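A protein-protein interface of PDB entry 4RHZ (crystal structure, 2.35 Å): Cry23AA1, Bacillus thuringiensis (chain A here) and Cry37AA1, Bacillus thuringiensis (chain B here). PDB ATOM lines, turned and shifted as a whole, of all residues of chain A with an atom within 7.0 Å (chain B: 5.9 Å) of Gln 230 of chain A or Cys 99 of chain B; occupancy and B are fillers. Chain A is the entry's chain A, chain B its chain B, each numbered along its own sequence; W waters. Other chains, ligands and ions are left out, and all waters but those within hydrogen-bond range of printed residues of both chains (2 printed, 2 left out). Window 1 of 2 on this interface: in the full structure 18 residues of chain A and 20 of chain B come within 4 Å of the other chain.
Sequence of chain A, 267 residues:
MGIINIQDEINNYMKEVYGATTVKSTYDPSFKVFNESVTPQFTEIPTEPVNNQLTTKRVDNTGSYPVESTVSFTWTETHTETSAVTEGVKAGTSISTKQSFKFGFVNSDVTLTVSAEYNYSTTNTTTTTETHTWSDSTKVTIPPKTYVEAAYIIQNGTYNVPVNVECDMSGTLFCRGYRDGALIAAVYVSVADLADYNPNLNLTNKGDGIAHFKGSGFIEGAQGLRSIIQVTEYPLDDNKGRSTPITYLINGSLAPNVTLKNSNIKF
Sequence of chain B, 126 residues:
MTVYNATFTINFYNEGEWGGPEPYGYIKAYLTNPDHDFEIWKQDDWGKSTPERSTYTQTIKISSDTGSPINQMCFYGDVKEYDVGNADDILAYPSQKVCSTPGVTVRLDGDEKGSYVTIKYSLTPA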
ATOM      1  N   ASN A  51       4.092 -18.437  27.327  1.00  0.00           N
ATOM      2  CA  ASN A  51       4.279 -17.169  28.010  1.00  0.00           C
ATOM      3  C   ASN A  51       3.273 -16.237  27.447  1.00  0.00           C
ATOM      4  O   ASN A  51       3.250 -16.022  26.257  1.00  0.00           O
ATOM      5  CB  ASN A  51       5.713 -16.601  27.771  1.00  0.00           C
ATOM      6  CG  ASN A  51       6.778 -17.283  28.674  1.00  0.00           C
ATOM      7  OD1 ASN A  51       6.445 -18.105  29.589  1.00  0.00           O
ATOM      8  ND2 ASN A  51       8.066 -16.923  28.463  1.00  0.00           N
ATOM      9  N   GLN A  53       1.806 -12.297  27.932  1.00  0.00           N
ATOM     10  CA  GLN A  53       2.004 -11.034  28.533  1.00  0.00           C
ATOM     11  C   GLN A  53       0.702 -10.434  29.010  1.00  0.00           C
ATOM     12  O   GLN A  53      -0.250 -10.297  28.228  1.00  0.00           O
ATOM     13  CB  GLN A  53       2.670 -10.126  27.523  1.00  0.00           C
ATOM     14  CG  GLN A  53       3.272  -8.981  28.228  1.00  0.00           C
ATOM     15  CD  GLN A  53       3.139  -7.760  27.464  1.00  0.00           C
ATOM     16  OE1 GLN A  53       2.058  -7.142  27.440  1.00  0.00           O
ATOM     17  NE2 GLN A  53       4.264  -7.355  26.795  1.00  0.00           N
ATOM     18  N   THR A  56       1.927  -4.169  31.384  1.00  0.00           N
ATOM     19  CA  THR A  56       3.239  -3.661  31.531  1.00  0.00           C
ATOM     20  C   THR A  56       3.203  -2.362  32.340  1.00  0.00           C
ATOM     21  O   THR A  56       2.211  -1.587  32.332  1.00  0.00           O
ATOM     22  CB  THR A  56       3.901  -3.409  30.157  1.00  0.00           C
ATOM     23  OG1 THR A  56       3.126  -2.399  29.536  1.00  0.00           O
ATOM     24  CG2 THR A  56       3.811  -4.608  29.251  1.00  0.00           C
ATOM     25  N   LYS A  57       4.310  -2.135  33.025  1.00  0.00           N
ATOM     26  CA  LYS A  57       4.480  -0.906  33.767  1.00  0.00           C
ATOM     27  C   LYS A  57       5.717  -0.221  33.193  1.00  0.00           C
ATOM     28  O   LYS A  57       6.805  -0.837  33.114  1.00  0.00           O
ATOM     29  CB  LYS A  57       4.631  -1.240  35.252  1.00  0.00           C
ATOM     30  CG  LYS A  57       3.288  -1.540  35.879  1.00  0.00           C
ATOM     31  CD  LYS A  57       3.233  -1.663  37.355  1.00  0.00           C
ATOM     32  CE  LYS A  57       1.743  -1.938  37.768  1.00  0.00           C
ATOM     33  NZ  LYS A  57       1.594  -2.094  39.237  1.00  0.00           N
ATOM     34  N   PHE A  73       3.077  -6.298  40.568  1.00  0.00           N
ATOM     35  CA  PHE A  73       2.032  -6.823  39.706  1.00  0.00           C
ATOM     36  C   PHE A  73       1.161  -7.765  40.485  1.00  0.00           C
ATOM     37  O   PHE A  73       1.617  -8.497  41.384  1.00  0.00           O
ATOM     38  CB  PHE A  73       2.658  -7.612  38.572  1.00  0.00           C
ATOM     39  CG  PHE A  73       3.474  -6.781  37.662  1.00  0.00           C
ATOM     40  CD1 PHE A  73       4.861  -6.798  37.740  1.00  0.00           C
ATOM     41  CD2 PHE A  73       2.860  -5.982  36.735  1.00  0.00           C
ATOM     42  CE1 PHE A  73       5.627  -6.027  36.864  1.00  0.00           C
ATOM     43  CE2 PHE A  73       3.608  -5.196  35.856  1.00  0.00           C
ATOM     44  CZ  PHE A  73       5.005  -5.229  35.920  1.00  0.00           C
ATOM     45  N   GLU A 149      10.385  -0.693  30.463  1.00  0.00           N
ATOM     46  CA  GLU A 149       9.075  -1.344  30.346  1.00  0.00           C
ATOM     47  C   GLU A 149       9.199  -2.654  31.105  1.00  0.00           C
ATOM     48  O   GLU A 149      10.035  -3.508  30.704  1.00  0.00           O
ATOM     49  CB  GLU A 149       8.727  -1.635  28.882  1.00  0.00           C
ATOM     50  CG  GLU A 149       7.917  -0.516  28.210  1.00  0.00           C
ATOM     51  CD  GLU A 149       7.921  -0.551  26.676  1.00  0.00           C
ATOM     52  OE1 GLU A 149       8.323  -1.570  26.087  1.00  0.00           O
ATOM     53  OE2 GLU A 149       7.547   0.460  26.042  1.00  0.00           O
ATOM     54  N   ALA A 150       8.433  -2.791  32.198  1.00  0.00           N
ATOM     55  CA  ALA A 150       8.460  -4.030  32.965  1.00  0.00           C
ATOM     56  C   ALA A 150       7.135  -4.724  32.598  1.00  0.00           C
ATOM     57  O   ALA A 150       6.022  -4.191  32.882  1.00  0.00           O
ATOM     58  CB  ALA A 150       8.580  -3.796  34.504  1.00  0.00           C
ATOM     59  N   ALA A 151       7.255  -5.831  31.879  1.00  0.00           N
ATOM     60  CA  ALA A 151       6.038  -6.596  31.429  1.00  0.00           C
ATOM     61  C   ALA A 151       5.853  -7.818  32.353  1.00  0.00           C
ATOM     62  O   ALA A 151       6.790  -8.538  32.642  1.00  0.00           O
ATOM     63  CB  ALA A 151       6.189  -7.024  29.944  1.00  0.00           C
ATOM     64  N   TYR A 152       4.638  -8.042  32.808  1.00  0.00           N
ATOM     65  CA  TYR A 152       4.338  -9.213  33.652  1.00  0.00           C
ATOM     66  C   TYR A 152       3.900 -10.375  32.757  1.00  0.00           C
ATOM     67  O   TYR A 152       2.949 -10.249  31.962  1.00  0.00           O
ATOM     68  CB  TYR A 152       3.204  -8.805  34.627  1.00  0.00           C
ATOM     69  CG  TYR A 152       2.989  -9.735  35.782  1.00  0.00           C
ATOM     70  CD1 TYR A 152       4.077 -10.290  36.460  1.00  0.00           C
ATOM     71  CD2 TYR A 152       1.704  -9.976  36.271  1.00  0.00           C
ATOM     72  CE1 TYR A 152       3.880 -11.091  37.559  1.00  0.00           C
ATOM     73  CE2 TYR A 152       1.504 -10.818  37.361  1.00  0.00           C
ATOM     74  CZ  TYR A 152       2.566 -11.340  37.984  1.00  0.00           C
ATOM     75  OH  TYR A 152       2.379 -12.097  39.083  1.00  0.00           O
ATOM     76  N   ILE A 153       4.632 -11.481  32.851  1.00  0.00           N
ATOM     77  CA  ILE A 153       4.450 -12.642  31.985  1.00  0.00           C
ATOM     78  C   ILE A 153       3.927 -13.804  32.858  1.00  0.00           C
ATOM     79  O   ILE A 153       4.536 -14.096  33.913  1.00  0.00           O
ATOM     80  CB  ILE A 153       5.801 -13.195  31.398  1.00  0.00           C
ATOM     81  CG1 ILE A 153       6.499 -12.307  30.321  1.00  0.00           C
ATOM     82  CG2 ILE A 153       5.577 -14.503  30.716  1.00  0.00           C
ATOM     83  CD1 ILE A 153       5.714 -11.177  29.830  1.00  0.00           C
ATOM     84  N   GLN A 155       3.333 -17.888  32.615  1.00  0.00           N
ATOM     85  CA  GLN A 155       3.636 -19.028  31.835  1.00  0.00           C
ATOM     86  C   GLN A 155       2.575 -20.142  32.112  1.00  0.00           C
ATOM     87  O   GLN A 155       2.554 -20.727  33.182  1.00  0.00           O
ATOM     88  CB  GLN A 155       5.047 -19.510  32.135  1.00  0.00           C
ATOM     89  CG  GLN A 155       5.457 -20.637  31.309  1.00  0.00           C
ATOM     90  CD  GLN A 155       6.898 -20.967  31.456  1.00  0.00           C
ATOM     91  OE1 GLN A 155       7.260 -22.016  32.006  1.00  0.00           O
ATOM     92  NE2 GLN A 155       7.770 -20.057  30.968  1.00  0.00           N
ATOM     93  N   ILE A 228       6.907 -14.320  35.426  1.00  0.00           N
ATOM     94  CA  ILE A 228       8.187 -13.748  35.092  1.00  0.00           C
ATOM     95  C   ILE A 228       7.955 -12.204  34.948  1.00  0.00           C
ATOM     96  O   ILE A 228       6.869 -11.754  34.491  1.00  0.00           O
ATOM     97  CB  ILE A 228       8.677 -14.335  33.772  1.00  0.00           C
ATOM     98  CG1 ILE A 228       9.094 -15.779  33.955  1.00  0.00           C
ATOM     99  CG2 ILE A 228       9.913 -13.570  33.235  1.00  0.00           C
ATOM    100  CD1 ILE A 228       9.281 -16.526  32.627  1.00  0.00           C
ATOM    101  N   ILE A 229       8.935 -11.401  35.382  1.00  0.00           N
ATOM    102  CA  ILE A 229       8.916  -9.942  35.132  1.00  0.00           C
ATOM    103  C   ILE A 229       9.945  -9.674  34.077  1.00  0.00           C
ATOM    104  O   ILE A 229      11.130  -9.970  34.258  1.00  0.00           O
ATOM    105  CB  ILE A 229       9.207  -9.157  36.384  1.00  0.00           C
ATOM    106  CG1 ILE A 229       8.004  -9.324  37.341  1.00  0.00           C
ATOM    107  CG2 ILE A 229       9.401  -7.684  36.031  1.00  0.00           C
ATOM    108  CD1 ILE A 229       8.259  -8.871  38.735  1.00  0.00           C
ATOM    109  N   GLN A 230       9.511  -9.175  32.936  1.00  0.00           N
ATOM    110  CA  GLN A 230      10.418  -9.070  31.840  1.00  0.00           C
ATOM    111  C   GLN A 230      10.728  -7.575  31.662  1.00  0.00           C
ATOM    112  O   GLN A 230       9.821  -6.760  31.419  1.00  0.00           O
ATOM    113  CB  GLN A 230       9.719  -9.642  30.572  1.00  0.00           C
ATOM    114  CG  GLN A 230      10.373  -9.315  29.258  1.00  0.00           C
ATOM    115  CD  GLN A 230       9.462  -9.567  28.062  1.00  0.00           C
ATOM    116  OE1 GLN A 230       9.174 -10.735  27.749  1.00  0.00           O
ATOM    117  NE2 GLN A 230       9.074  -8.496  27.339  1.00  0.00           N
ATOM    118  N   VAL A 231      12.003  -7.216  31.772  1.00  0.00           N
ATOM    119  CA  VAL A 231      12.359  -5.768  31.841  1.00  0.00           C
ATOM    120  C   VAL A 231      13.172  -5.352  30.658  1.00  0.00           C
ATOM    121  O   VAL A 231      14.280  -5.893  30.407  1.00  0.00           O
ATOM    122  CB  VAL A 231      13.110  -5.422  33.134  1.00  0.00           C
ATOM    123  CG1 VAL A 231      13.447  -3.872  33.171  1.00  0.00           C
ATOM    124  CG2 VAL A 231      12.232  -5.776  34.387  1.00  0.00           C
ATOM    125  N   THR A 232      12.629  -4.377  29.935  1.00  0.00           N
ATOM    126  CA  THR A 232      13.369  -3.722  28.843  1.00  0.00           C
ATOM    127  C   THR A 232      13.799  -2.269  29.154  1.00  0.00           C
ATOM    128  O   THR A 232      12.949  -1.424  29.473  1.00  0.00           O
ATOM    129  CB  THR A 232      12.518  -3.736  27.512  1.00  0.00           C
ATOM    130  OG1 THR A 232      12.223  -5.116  27.175  1.00  0.00           O
ATOM    131  CG2 THR A 232      13.302  -3.188  26.406  1.00  0.00           C
ATOM    132  N   THR A 247      17.065  -6.161  27.221  1.00  0.00           N
ATOM    133  CA  THR A 247      15.982  -6.869  27.881  1.00  0.00           C
ATOM    134  C   THR A 247      16.504  -7.963  28.809  1.00  0.00           C
ATOM    135  O   THR A 247      17.282  -8.793  28.378  1.00  0.00           O
ATOM    136  CB  THR A 247      15.028  -7.483  26.870  1.00  0.00           C
ATOM    137  OG1 THR A 247      14.378  -6.447  26.092  1.00  0.00           O
ATOM    138  CG2 THR A 247      13.946  -8.380  27.598  1.00  0.00           C
ATOM    139  N   TYR A 248      16.107  -7.956  30.081  1.00  0.00           N
ATOM    140  CA  TYR A 248      16.497  -9.068  30.990  1.00  0.00           C
ATOM    141  C   TYR A 248      15.245  -9.570  31.756  1.00  0.00           C
ATOM    142  O   TYR A 248      14.226  -8.881  31.803  1.00  0.00           O
ATOM    143  CB  TYR A 248      17.615  -8.659  31.993  1.00  0.00           C
ATOM    144  CG  TYR A 248      17.259  -7.440  32.834  1.00  0.00           C
ATOM    145  CD1 TYR A 248      16.782  -7.575  34.138  1.00  0.00           C
ATOM    146  CD2 TYR A 248      17.411  -6.143  32.326  1.00  0.00           C
ATOM    147  CE1 TYR A 248      16.426  -6.457  34.897  1.00  0.00           C
ATOM    148  CE2 TYR A 248      17.080  -4.994  33.095  1.00  0.00           C
ATOM    149  CZ  TYR A 248      16.604  -5.160  34.373  1.00  0.00           C
ATOM    150  OH  TYR A 248      16.229  -4.043  35.117  1.00  0.00           O
ATOM    151  N   LEU A 249      15.300 -10.775  32.320  1.00  0.00           N
ATOM    152  CA  LEU A 249      14.094 -11.381  32.927  1.00  0.00           C
ATOM    153  C   LEU A 249      14.341 -11.719  34.351  1.00  0.00           C
ATOM    154  O   LEU A 249      15.372 -12.285  34.681  1.00  0.00           O
ATOM    155  CB  LEU A 249      13.733 -12.651  32.200  1.00  0.00           C
ATOM    156  CG  LEU A 249      13.514 -12.537  30.686  1.00  0.00           C
ATOM    157  CD1 LEU A 249      13.510 -13.937  30.084  1.00  0.00           C
ATOM    158  CD2 LEU A 249      12.306 -11.806  30.351  1.00  0.00           C
ATOM    159  N   ILE A 250      13.404 -11.346  35.205  1.00  0.00           N
ATOM    160  CA  ILE A 250      13.514 -11.614  36.618  1.00  0.00           C
ATOM    161  C   ILE A 250      12.406 -12.664  36.995  1.00  0.00           C
ATOM    162  O   ILE A 250      11.216 -12.438  36.744  1.00  0.00           O
ATOM    163  CB  ILE A 250      13.236 -10.308  37.394  1.00  0.00           C
ATOM    164  CG1 ILE A 250      14.292  -9.237  37.088  1.00  0.00           C
ATOM    165  CG2 ILE A 250      13.127 -10.576  38.943  1.00  0.00           C
ATOM    166  CD1 ILE A 250      13.757  -7.857  37.435  1.00  0.00           C
ATOM    167  N   TYR B  30      15.116 -10.919  18.886  1.00  0.00           N
ATOM    168  CA  TYR B  30      16.443 -10.486  19.290  1.00  0.00           C
ATOM    169  C   TYR B  30      16.794 -11.255  20.534  1.00  0.00           C
ATOM    170  O   TYR B  30      15.888 -11.707  21.257  1.00  0.00           O
ATOM    171  CB  TYR B  30      16.483  -8.948  19.582  1.00  0.00           C
ATOM    172  CG  TYR B  30      15.558  -8.414  20.711  1.00  0.00           C
ATOM    173  CD1 TYR B  30      16.019  -8.267  21.989  1.00  0.00           C
ATOM    174  CD2 TYR B  30      14.274  -8.003  20.453  1.00  0.00           C
ATOM    175  CE1 TYR B  30      15.198  -7.808  23.029  1.00  0.00           C
ATOM    176  CE2 TYR B  30      13.454  -7.485  21.461  1.00  0.00           C
ATOM    177  CZ  TYR B  30      13.937  -7.401  22.751  1.00  0.00           C
ATOM    178  OH  TYR B  30      13.163  -6.935  23.789  1.00  0.00           O
ATOM    179  N   GLN B  72      17.611 -17.106  26.104  1.00  0.00           N
ATOM    180  CA  GLN B  72      16.572 -16.080  26.050  1.00  0.00           C
ATOM    181  C   GLN B  72      16.342 -15.579  24.631  1.00  0.00           C
ATOM    182  O   GLN B  72      17.285 -15.314  23.902  1.00  0.00           O
ATOM    183  CB  GLN B  72      16.989 -14.861  26.923  1.00  0.00           C
ATOM    184  CG  GLN B  72      16.065 -13.659  26.924  1.00  0.00           C
ATOM    185  CD  GLN B  72      16.533 -12.514  27.900  1.00  0.00           C
ATOM    186  OE1 GLN B  72      16.720 -12.724  29.118  1.00  0.00           O
ATOM    187  NE2 GLN B  72      16.732 -11.324  27.346  1.00  0.00           N
ATOM    188  N   MET B  73      15.084 -15.341  24.264  1.00  0.00           N
ATOM    189  CA  MET B  73      14.841 -14.767  22.989  1.00  0.00           C
ATOM    190  C   MET B  73      13.570 -14.014  23.097  1.00  0.00           C
ATOM    191  O   MET B  73      12.647 -14.467  23.796  1.00  0.00           O
ATOM    192  CB  MET B  73      14.827 -15.919  21.967  1.00  0.00           C
ATOM    193  CG  MET B  73      14.576 -15.475  20.569  1.00  0.00           C
ATOM    194  SD  MET B  73      15.626 -16.218  19.253  1.00  0.00           S
ATOM    195  CE  MET B  73      16.506 -17.545  19.833  1.00  0.00           C
ATOM    196  N   CYS B  74      13.497 -12.846  22.451  1.00  0.00           N
ATOM    197  CA  CYS B  74      12.388 -11.973  22.618  1.00  0.00           C
ATOM    198  C   CYS B  74      11.771 -11.780  21.279  1.00  0.00           C
ATOM    199  O   CYS B  74      12.495 -11.717  20.306  1.00  0.00           O
ATOM    200  CB  CYS B  74      12.856 -10.637  23.227  1.00  0.00           C
ATOM    201  SG  CYS B  74      13.550 -10.829  24.890  1.00  0.00           S
ATOM    202  N   PHE B  75      10.436 -11.677  21.181  1.00  0.00           N
ATOM    203  CA  PHE B  75       9.808 -11.702  19.857  1.00  0.00           C
ATOM    204  C   PHE B  75       8.789 -10.605  19.791  1.00  0.00           C
ATOM    205  O   PHE B  75       8.165 -10.279  20.814  1.00  0.00           O
ATOM    206  CB  PHE B  75       9.085 -13.044  19.614  1.00  0.00           C
ATOM    207  CG  PHE B  75       9.967 -14.251  19.651  1.00  0.00           C
ATOM    208  CD1 PHE B  75      10.129 -14.973  20.832  1.00  0.00           C
ATOM    209  CD2 PHE B  75      10.595 -14.708  18.499  1.00  0.00           C
ATOM    210  CE1 PHE B  75      10.967 -16.110  20.886  1.00  0.00           C
ATOM    211  CE2 PHE B  75      11.399 -15.910  18.503  1.00  0.00           C
ATOM    212  CZ  PHE B  75      11.627 -16.585  19.696  1.00  0.00           C
ATOM    213  N   LYS B  97       6.448  -6.975  23.101  1.00  0.00           N
ATOM    214  CA  LYS B  97       7.555  -7.872  23.101  1.00  0.00           C
ATOM    215  C   LYS B  97       7.363  -8.971  24.133  1.00  0.00           C
ATOM    216  O   LYS B  97       7.032  -8.669  25.314  1.00  0.00           O
ATOM    217  CB  LYS B  97       8.859  -7.111  23.469  1.00  0.00           C
ATOM    218  CG  LYS B  97       9.550  -6.473  22.235  1.00  0.00           C
ATOM    219  CD  LYS B  97       8.848  -5.166  21.863  1.00  0.00           C
ATOM    220  CE  LYS B  97       9.639  -4.391  20.742  1.00  0.00           C
ATOM    221  NZ  LYS B  97       8.753  -3.332  20.108  1.00  0.00           N
ATOM    222  N   VAL B  98       7.536 -10.241  23.723  1.00  0.00           N
ATOM    223  CA  VAL B  98       7.419 -11.375  24.706  1.00  0.00           C
ATOM    224  C   VAL B  98       8.604 -12.266  24.530  1.00  0.00           C
ATOM    225  O   VAL B  98       8.894 -12.656  23.409  1.00  0.00           O
ATOM    226  CB  VAL B  98       6.054 -12.218  24.541  1.00  0.00           C
ATOM    227  CG1 VAL B  98       5.831 -13.194  25.728  1.00  0.00           C
ATOM    228  CG2 VAL B  98       4.828 -11.270  24.460  1.00  0.00           C
ATOM    229  N   CYS B  99       9.293 -12.597  25.621  1.00  0.00           N
ATOM    230  CA  CYS B  99      10.497 -13.411  25.561  1.00  0.00           C
ATOM    231  C   CYS B  99      10.236 -14.822  26.187  1.00  0.00           C
ATOM    232  O   CYS B  99       9.379 -14.968  27.024  1.00  0.00           O
ATOM    233  CB  CYS B  99      11.634 -12.701  26.394  1.00  0.00           C
ATOM    234  SG  CYS B  99      11.779 -10.867  25.965  1.00  0.00           S
ATOM    235  N   SER B 100      11.050 -15.809  25.841  1.00  0.00           N
ATOM    236  CA  SER B 100      11.051 -17.080  26.543  1.00  0.00           C
ATOM    237  C   SER B 100      12.420 -17.762  26.430  1.00  0.00           C
ATOM    238  O   SER B 100      13.204 -17.429  25.560  1.00  0.00           O
ATOM    239  CB  SER B 100      10.018 -18.012  25.879  1.00  0.00           C
ATOM    240  OG  SER B 100      10.326 -18.132  24.492  1.00  0.00           O
ATOM    241  N   THR B 101      12.672 -18.745  27.279  1.00  0.00           N
ATOM    242  CA  THR B 101      13.739 -19.726  27.067  1.00  0.00           C
ATOM    243  C   THR B 101      13.372 -20.761  25.958  1.00  0.00           C
ATOM    244  O   THR B 101      12.208 -20.957  25.679  1.00  0.00           O
ATOM    245  CB  THR B 101      13.911 -20.535  28.347  1.00  0.00           C
ATOM    246  OG1 THR B 101      12.637 -21.139  28.650  1.00  0.00           O
ATOM    247  CG2 THR B 101      14.327 -19.613  29.538  1.00  0.00           C
ATOM    248  N   VAL B 106       5.981 -18.552  22.973  1.00  0.00           N
ATOM    249  CA  VAL B 106       5.352 -17.290  23.323  1.00  0.00           C
ATOM    250  C   VAL B 106       4.127 -17.032  22.459  1.00  0.00           C
ATOM    251  O   VAL B 106       4.099 -17.440  21.309  1.00  0.00           O
ATOM    252  CB  VAL B 106       6.333 -15.983  23.164  1.00  0.00           C
ATOM    253  CG1 VAL B 106       7.630 -16.103  23.906  1.00  0.00           C
ATOM    254  CG2 VAL B 106       6.538 -15.614  21.686  1.00  0.00           C
HETATM  255  O   HOH W   1      17.811 -12.218  31.835  1.00  0.00           O
HETATM  256  O   HOH W   2       6.330  -5.902  25.747  1.00  0.00           O
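NE2 of Gln 53 of chain A is in hydrogen-bond range of O of Lys 97 of chain B, at 3.4 Å. The side-chain hydroxyl (OG1) of Thr 247 of chain A sits at hydrogen-bond distance from the side-chain hydroxyl (OH) of Tyr 30 of chain B (2.6 Å). The side-chain amide nitrogen (NE2) of Gln 230 of chain A sits at hydrogen-bond distance from the backbone carbonyl oxygen (O) of Lys 97 of chain B. ND2 of Asn 51 of chain A sits at hydrogen-bond distance from O of Cys 99 of chain B (2.8 Å). NE2 of Gln 72 of chain B is in hydrogen-bond range of O of Thr 247 of chain A (2.8 Å). The side-chain amide oxygen of Gln 230 of chain A sits at hydrogen-bond distance from the backbone NH of Cys 99 of chain B (2.8 Å).
The backbone NH of Ala 151 of chain A lies within hydrogen-bond range of the backbone carbonyl oxygen of Gln 230 of chain A (2.8 Å). The backbone NH (N) of Thr 232 of chain A is in hydrogen-bond range of the backbone carbonyl oxygen (O) of Glu 149 of chain A, 2.8 Å away. The backbone NH of Ser 100 of chain B is in hydrogen-bond range of the backbone carbonyl oxygen of Met 73 of chain B (2.9 Å). The side-chain hydroxyl (OG1) of Thr 232 of chain A lies within hydrogen-bond range of the side-chain hydroxyl (OG1) of Thr 247 of chain A (2.8 Å). SG of Cys 74 of chain B forms a disulfide with SG of Cys 99 of chain B, at 2.1 Å. The side-chain amide oxygen (OD1) of Asn 51 of chain A is in hydrogen-bond range of the side-chain amide nitrogen (NE2) of Gln 155 of chain A, 2.7 Å away.
Among the printed residues, merely in contact across the chains: Asn 51 of chain A with Val 98 of chain B (3.9 Å), Asn 51 of chain A with Ser 100 of chain B (3.4 Å), Asn 51 of chain A with Val 106 of chain B (3.8 Å), Gln 53 of chain A with Val 98 of chain B (3.9 Å), Gln 230 of chain A with Val 98 of chain B (3.6 Å), Thr 232 of chain A with Tyr 30 of chain B (3.96 Å), Thr 247 of chain A with Cys 74 of chain B (3.7 Å), Thr 247 of chain A with Cys 99 of chain B (3.7 Å) and Leu 249 of chain A with Gln 72 of chain B (3.6 Å).
Of the printed residues of chain B, Gln 230 of chain A touches Lys 97, Val 98 and Cys 99. Of the printed residues of chain A, Tyr 30 of chain B touches Thr 232 and Thr 247. Printed residues of chain A within 4 Å of Val 98 of chain B: Asn 51 (3.9 Å), Gln 53 (3.9 Å) and Gln 230 (3.6 Å). Of the printed residues of chain B, Gln 53 of chain A touches Lys 97 and Val 98. Phe 75 of chain B touches none of the printed residues of chain A. Phe 73 of chain A touches none of the printed residues of chain B. The nearest residue of chain B that does not touch Gln 230 of chain A is Cys 74 of chain B (5.2 Å). The nearest residue of chain A that does not touch Cys 99 of chain B is Leu 249 of chain A (4.1 Å).
Of the 20 printed residues of chain A, 6 touch a printed residue of chain B. Hydrophobic or aromatic side chains of chain A that line the printed part of chain B: Leu 249. Hydrophobic or aromatic side chains of chain B within 4 Å of the printed part of chain A: Tyr 30 and Val 98. Among the printed residues, 15 pairs touch across the chains. Among the printed residues, no Asp or Glu carboxylate lies within 4 Å of a Lys or Arg side-chain nitrogen of the other chain.
Water W2 lies within hydrogen-bond range of NE2 of Gln 53 of chain A and N of Lys 97 of chain B. Water W1 lies within hydrogen-bond range of N of Leu 249 of chain A (2.9 Å) and OE1 of Gln 72 of chain B (3.0 Å).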
